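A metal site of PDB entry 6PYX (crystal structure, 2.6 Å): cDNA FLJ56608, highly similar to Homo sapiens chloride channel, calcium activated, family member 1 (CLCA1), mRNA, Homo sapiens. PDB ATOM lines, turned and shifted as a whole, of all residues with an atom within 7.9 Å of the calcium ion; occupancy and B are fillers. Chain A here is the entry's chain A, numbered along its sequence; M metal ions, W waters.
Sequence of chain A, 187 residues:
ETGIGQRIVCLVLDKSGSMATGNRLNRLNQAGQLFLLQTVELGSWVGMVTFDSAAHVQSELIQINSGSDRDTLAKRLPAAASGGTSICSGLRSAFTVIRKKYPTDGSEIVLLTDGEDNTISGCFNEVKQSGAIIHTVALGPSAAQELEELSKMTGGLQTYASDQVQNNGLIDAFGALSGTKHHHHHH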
ATOM      1  N   ASP A  14      18.942   1.032  -9.811  1.00  0.00           N
ATOM      2  CA  ASP A  14      18.275   0.392 -10.939  1.00  0.00           C
ATOM      3  C   ASP A  14      19.314  -0.102 -11.938  1.00  0.00           C
ATOM      4  O   ASP A  14      19.853   0.686 -12.721  1.00  0.00           O
ATOM      5  CB  ASP A  14      17.330   1.378 -11.594  1.00  0.00           C
ATOM      6  CG  ASP A  14      16.347   0.722 -12.532  1.00  0.00           C
ATOM      7  OD1 ASP A  14      16.583  -0.443 -12.912  1.00  0.00           O
ATOM      8  OD2 ASP A  14      15.339   1.384 -12.891  1.00  0.00           O
ATOM      9  N   LYS A  15      19.602  -1.403 -11.931  1.00  0.00           N
ATOM     10  CA  LYS A  15      20.468  -2.023 -12.929  1.00  0.00           C
ATOM     11  C   LYS A  15      19.673  -2.703 -14.038  1.00  0.00           C
ATOM     12  O   LYS A  15      20.271  -3.385 -14.877  1.00  0.00           O
ATOM     13  CB  LYS A  15      21.410  -3.040 -12.278  1.00  0.00           C
ATOM     14  CG  LYS A  15      20.706  -4.295 -11.749  1.00  0.00           C
ATOM     15  CD  LYS A  15      21.608  -5.520 -11.669  1.00  0.00           C
ATOM     16  CE  LYS A  15      21.771  -6.173 -13.021  1.00  0.00           C
ATOM     17  NZ  LYS A  15      20.476  -6.259 -13.737  1.00  0.00           N
ATOM     18  N   SER A  16      18.350  -2.542 -14.065  1.00  0.00           N
ATOM     19  CA  SER A  16      17.504  -3.303 -14.968  1.00  0.00           C
ATOM     20  C   SER A  16      17.821  -2.970 -16.429  1.00  0.00           C
ATOM     21  O   SER A  16      18.553  -2.018 -16.738  1.00  0.00           O
ATOM     22  CB  SER A  16      16.034  -3.042 -14.677  1.00  0.00           C
ATOM     23  OG  SER A  16      15.615  -1.791 -15.197  1.00  0.00           O
ATOM     24  N   GLY A  17      17.216  -3.753 -17.332  1.00  0.00           N
ATOM     25  CA  GLY A  17      17.605  -3.723 -18.730  1.00  0.00           C
ATOM     26  C   GLY A  17      17.370  -2.377 -19.406  1.00  0.00           C
ATOM     27  O   GLY A  17      18.157  -1.942 -20.251  1.00  0.00           O
ATOM     28  N   SER A  18      16.269  -1.718 -19.055  1.00  0.00           N
ATOM     29  CA  SER A  18      15.987  -0.413 -19.641  1.00  0.00           C
ATOM     30  C   SER A  18      17.091   0.584 -19.344  1.00  0.00           C
ATOM     31  O   SER A  18      17.246   1.553 -20.086  1.00  0.00           O
ATOM     32  CB  SER A  18      14.647   0.120 -19.145  1.00  0.00           C
ATOM     33  OG  SER A  18      14.770   0.713 -17.864  1.00  0.00           O
ATOM     34  N   MET A  19      17.870   0.338 -18.293  1.00  0.00           N
ATOM     35  CA  MET A  19      18.926   1.264 -17.921  1.00  0.00           C
ATOM     36  C   MET A  19      20.116   1.190 -18.856  1.00  0.00           C
ATOM     37  O   MET A  19      21.016   2.029 -18.740  1.00  0.00           O
ATOM     38  CB  MET A  19      19.360   1.001 -16.481  1.00  0.00           C
ATOM     39  CG  MET A  19      18.317   1.414 -15.452  1.00  0.00           C
ATOM     40  SD  MET A  19      18.153   3.199 -15.269  1.00  0.00           S
ATOM     41  CE  MET A  19      19.741   3.570 -14.539  1.00  0.00           C
ATOM     42  N   ALA A  20      20.168   0.231 -19.784  1.00  0.00           N
ATOM     43  CA  ALA A  20      21.246   0.244 -20.765  1.00  0.00           C
ATOM     44  C   ALA A  20      21.040   1.270 -21.853  1.00  0.00           C
ATOM     45  O   ALA A  20      21.959   1.482 -22.668  1.00  0.00           O
ATOM     46  CB  ALA A  20      21.414  -1.132 -21.404  1.00  0.00           C
ATOM     47  N   ARG A  24      21.991   6.293 -19.025  1.00  0.00           N
ATOM     48  CA  ARG A  24      21.347   6.155 -17.726  1.00  0.00           C
ATOM     49  C   ARG A  24      22.269   5.467 -16.732  1.00  0.00           C
ATOM     50  O   ARG A  24      22.445   5.947 -15.610  1.00  0.00           O
ATOM     51  CB  ARG A  24      20.030   5.382 -17.871  1.00  0.00           C
ATOM     52  CG  ARG A  24      19.178   5.901 -18.999  1.00  0.00           C
ATOM     53  CD  ARG A  24      17.947   5.065 -19.171  1.00  0.00           C
ATOM     54  NE  ARG A  24      16.958   5.701 -20.028  1.00  0.00           N
ATOM     55  CZ  ARG A  24      15.680   5.345 -20.085  1.00  0.00           C
ATOM     56  NH1 ARG A  24      15.233   4.359 -19.324  1.00  0.00           N
ATOM     57  NH2 ARG A  24      14.857   5.999 -20.877  1.00  0.00           N
ATOM     58  N   PHE A  51      19.167  -3.717  -8.224  1.00  0.00           N
ATOM     59  CA  PHE A  51      17.945  -4.467  -8.465  1.00  0.00           C
ATOM     60  C   PHE A  51      17.648  -4.558  -9.950  1.00  0.00           C
ATOM     61  O   PHE A  51      17.890  -3.620 -10.714  1.00  0.00           O
ATOM     62  CB  PHE A  51      16.732  -3.867  -7.720  1.00  0.00           C
ATOM     63  CG  PHE A  51      16.299  -2.486  -8.204  1.00  0.00           C
ATOM     64  CD1 PHE A  51      15.531  -2.338  -9.348  1.00  0.00           C
ATOM     65  CD2 PHE A  51      16.622  -1.348  -7.478  1.00  0.00           C
ATOM     66  CE1 PHE A  51      15.136  -1.090  -9.783  1.00  0.00           C
ATOM     67  CE2 PHE A  51      16.223  -0.110  -7.915  1.00  0.00           C
ATOM     68  CZ  PHE A  51      15.471   0.023  -9.068  1.00  0.00           C
ATOM     69  N   ASP A  52      17.120  -5.705 -10.350  1.00  0.00           N
ATOM     70  CA  ASP A  52      16.508  -5.864 -11.654  1.00  0.00           C
ATOM     71  C   ASP A  52      15.116  -6.434 -11.427  1.00  0.00           C
ATOM     72  O   ASP A  52      14.236  -5.739 -10.930  1.00  0.00           O
ATOM     73  CB  ASP A  52      17.349  -6.737 -12.595  1.00  0.00           C
ATOM     74  CG  ASP A  52      18.002  -7.941 -11.896  1.00  0.00           C
ATOM     75  OD1 ASP A  52      17.324  -8.648 -11.121  1.00  0.00           O
ATOM     76  OD2 ASP A  52      19.210  -8.164 -12.105  1.00  0.00           O
ATOM     77  N   GLY A  83      17.959  -7.282 -17.351  1.00  0.00           N
ATOM     78  CA  GLY A  83      16.956  -7.981 -16.559  1.00  0.00           C
ATOM     79  C   GLY A  83      15.679  -7.183 -16.398  1.00  0.00           C
ATOM     80  O   GLY A  83      15.535  -6.044 -16.864  1.00  0.00           O
ATOM     81  N   GLY A  84      14.731  -7.798 -15.710  1.00  0.00           N
ATOM     82  CA  GLY A  84      13.449  -7.195 -15.431  1.00  0.00           C
ATOM     83  C   GLY A  84      13.586  -6.036 -14.463  1.00  0.00           C
ATOM     84  O   GLY A  84      14.674  -5.671 -14.035  1.00  0.00           O
ATOM     85  N   THR A  85      12.432  -5.430 -14.126  1.00  0.00           N
ATOM     86  CA  THR A  85      12.376  -4.218 -13.320  1.00  0.00           C
ATOM     87  C   THR A  85      11.339  -4.370 -12.209  1.00  0.00           C
ATOM     88  O   THR A  85      10.185  -4.681 -12.486  1.00  0.00           O
ATOM     89  CB  THR A  85      12.018  -2.989 -14.159  1.00  0.00           C
ATOM     90  OG1 THR A  85      13.099  -2.689 -15.042  1.00  0.00           O
ATOM     91  CG2 THR A  85      11.788  -1.811 -13.259  1.00  0.00           C
ATOM     92  N   SER A  86      11.752  -4.128 -10.973  1.00  0.00           N
ATOM     93  CA  SER A  86      10.825  -4.172  -9.853  1.00  0.00           C
ATOM     94  C   SER A  86      11.426  -3.281  -8.754  1.00  0.00           C
ATOM     95  O   SER A  86      12.291  -3.709  -7.978  1.00  0.00           O
ATOM     96  CB  SER A  86      10.589  -5.594  -9.394  1.00  0.00           C
ATOM     97  OG  SER A  86      10.174  -5.639  -8.032  1.00  0.00           O
ATOM     98  N   ILE A  87      10.974  -2.027  -8.738  1.00  0.00           N
ATOM     99  CA  ILE A  87      11.472  -1.070  -7.767  1.00  0.00           C
ATOM    100  C   ILE A  87      11.217  -1.581  -6.371  1.00  0.00           C
ATOM    101  O   ILE A  87      12.050  -1.417  -5.464  1.00  0.00           O
ATOM    102  CB  ILE A  87      10.832   0.300  -8.027  1.00  0.00           C
ATOM    103  CG1 ILE A  87      11.371   0.909  -9.331  1.00  0.00           C
ATOM    104  CG2 ILE A  87      11.032   1.234  -6.864  1.00  0.00           C
ATOM    105  CD1 ILE A  87      11.278   2.422  -9.437  1.00  0.00           C
ATOM    106  N   THR A 113      16.844   5.505 -10.437  1.00  0.00           N
ATOM    107  CA  THR A 113      16.093   4.701 -11.383  1.00  0.00           C
ATOM    108  C   THR A 113      15.644   5.577 -12.544  1.00  0.00           C
ATOM    109  O   THR A 113      15.599   6.804 -12.446  1.00  0.00           O
ATOM    110  CB  THR A 113      14.892   4.027 -10.706  1.00  0.00           C
ATOM    111  OG1 THR A 113      14.045   3.449 -11.708  1.00  0.00           O
ATOM    112  CG2 THR A 113      14.110   5.041  -9.891  1.00  0.00           C
ATOM    113  N   ASP A 114      15.354   4.926 -13.672  1.00  0.00           N
ATOM    114  CA  ASP A 114      14.712   5.610 -14.792  1.00  0.00           C
ATOM    115  C   ASP A 114      13.205   5.687 -14.611  1.00  0.00           C
ATOM    116  O   ASP A 114      12.527   6.378 -15.389  1.00  0.00           O
ATOM    117  CB  ASP A 114      15.093   4.939 -16.117  1.00  0.00           C
ATOM    118  CG  ASP A 114      14.585   3.505 -16.245  1.00  0.00           C
ATOM    119  OD1 ASP A 114      13.946   3.002 -15.297  1.00  0.00           O
ATOM    120  OD2 ASP A 114      14.803   2.886 -17.300  1.00  0.00           O
ATOM    121  N   GLY A 115      12.670   5.007 -13.590  1.00  0.00           N
ATOM    122  CA  GLY A 115      11.289   5.085 -13.209  1.00  0.00           C
ATOM    123  C   GLY A 115      10.342   4.253 -14.042  1.00  0.00           C
ATOM    124  O   GLY A 115       9.147   4.238 -13.749  1.00  0.00           O
ATOM    125  N   GLU A 116      10.844   3.542 -15.050  1.00  0.00           N
ATOM    126  CA  GLU A 116       9.983   2.798 -15.953  1.00  0.00           C
ATOM    127  C   GLU A 116       9.512   1.507 -15.265  1.00  0.00           C
ATOM    128  O   GLU A 116       9.931   0.399 -15.592  1.00  0.00           O
ATOM    129  CB  GLU A 116      10.703   2.545 -17.260  1.00  0.00           C
ATOM    130  CG  GLU A 116      11.215   3.852 -17.829  1.00  0.00           C
ATOM    131  CD  GLU A 116      11.913   3.698 -19.147  1.00  0.00           C
ATOM    132  OE1 GLU A 116      12.085   2.548 -19.594  1.00  0.00           O
ATOM    133  OE2 GLU A 116      12.278   4.730 -19.740  1.00  0.00           O
ATOM    134  N   ASP A 117       8.615   1.685 -14.296  1.00  0.00           N
ATOM    135  CA  ASP A 117       8.040   0.577 -13.538  1.00  0.00           C
ATOM    136  C   ASP A 117       6.651   0.984 -13.086  1.00  0.00           C
ATOM    137  O   ASP A 117       6.461   2.064 -12.518  1.00  0.00           O
ATOM    138  CB  ASP A 117       8.918   0.209 -12.336  1.00  0.00           C
ATOM    139  CG  ASP A 117       8.315  -0.894 -11.479  1.00  0.00           C
ATOM    140  OD1 ASP A 117       7.237  -1.418 -11.784  1.00  0.00           O
ATOM    141  OD2 ASP A 117       8.949  -1.259 -10.473  1.00  0.00           O
HETATM  142 CA    CA M   1      13.640  -0.789 -16.224  1.00  0.00          CA
HETATM  143  O   HOH W   1      10.893  -0.658 -18.137  1.00  0.00           O
HETATM  144  O   HOH W   2      13.837   0.912 -14.518  1.00  0.00           O
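The backbone NH (N) of Asp 114 lies close to the side-chain sulfur (SD) of Met 19, 3.7 Å away.
The side-chain carboxylate (OD2) of Asp 114 is in salt-bridge range of the guanidinium group (NH1) of Arg 24 (2.5 Å).
The backbone NH (N) of Ser 16 sits at hydrogen-bond distance from the side-chain carboxylate (OD1) of Asp 14.
The guanidinium group (NH1) of Arg 24 is in salt-bridge range of the side-chain carboxylate (OE2) of Glu 116 (3.0 Å).
The side-chain carboxylate (OD1) of Asp 114 lies within hydrogen-bond range of the backbone NH (N) of Glu 116 (3.2 Å).
Asp 114 touches the calcium ion (OD1 to CA, 3.9 Å).
Glu 116 touches the calcium ion (O to CA, 3.9 Å).
Five residues have an atom within 4 Å of the calcium ion: Ser 16, Ser 18, Thr 85, Asp 114 and Glu 116.
The nearest printed residue that does not touch the calcium ion is Asp 14 (4.3 Å).
The calcium ion is bound by the side-chain hydroxyl of Thr 85 (2.3 Å), water W2 (2.4 Å), the side-chain hydroxyl of Ser 16 (2.4 Å) and the side-chain hydroxyl of Ser 18 (2.5 Å).
The calcium ion has four donor atoms within binding distance.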
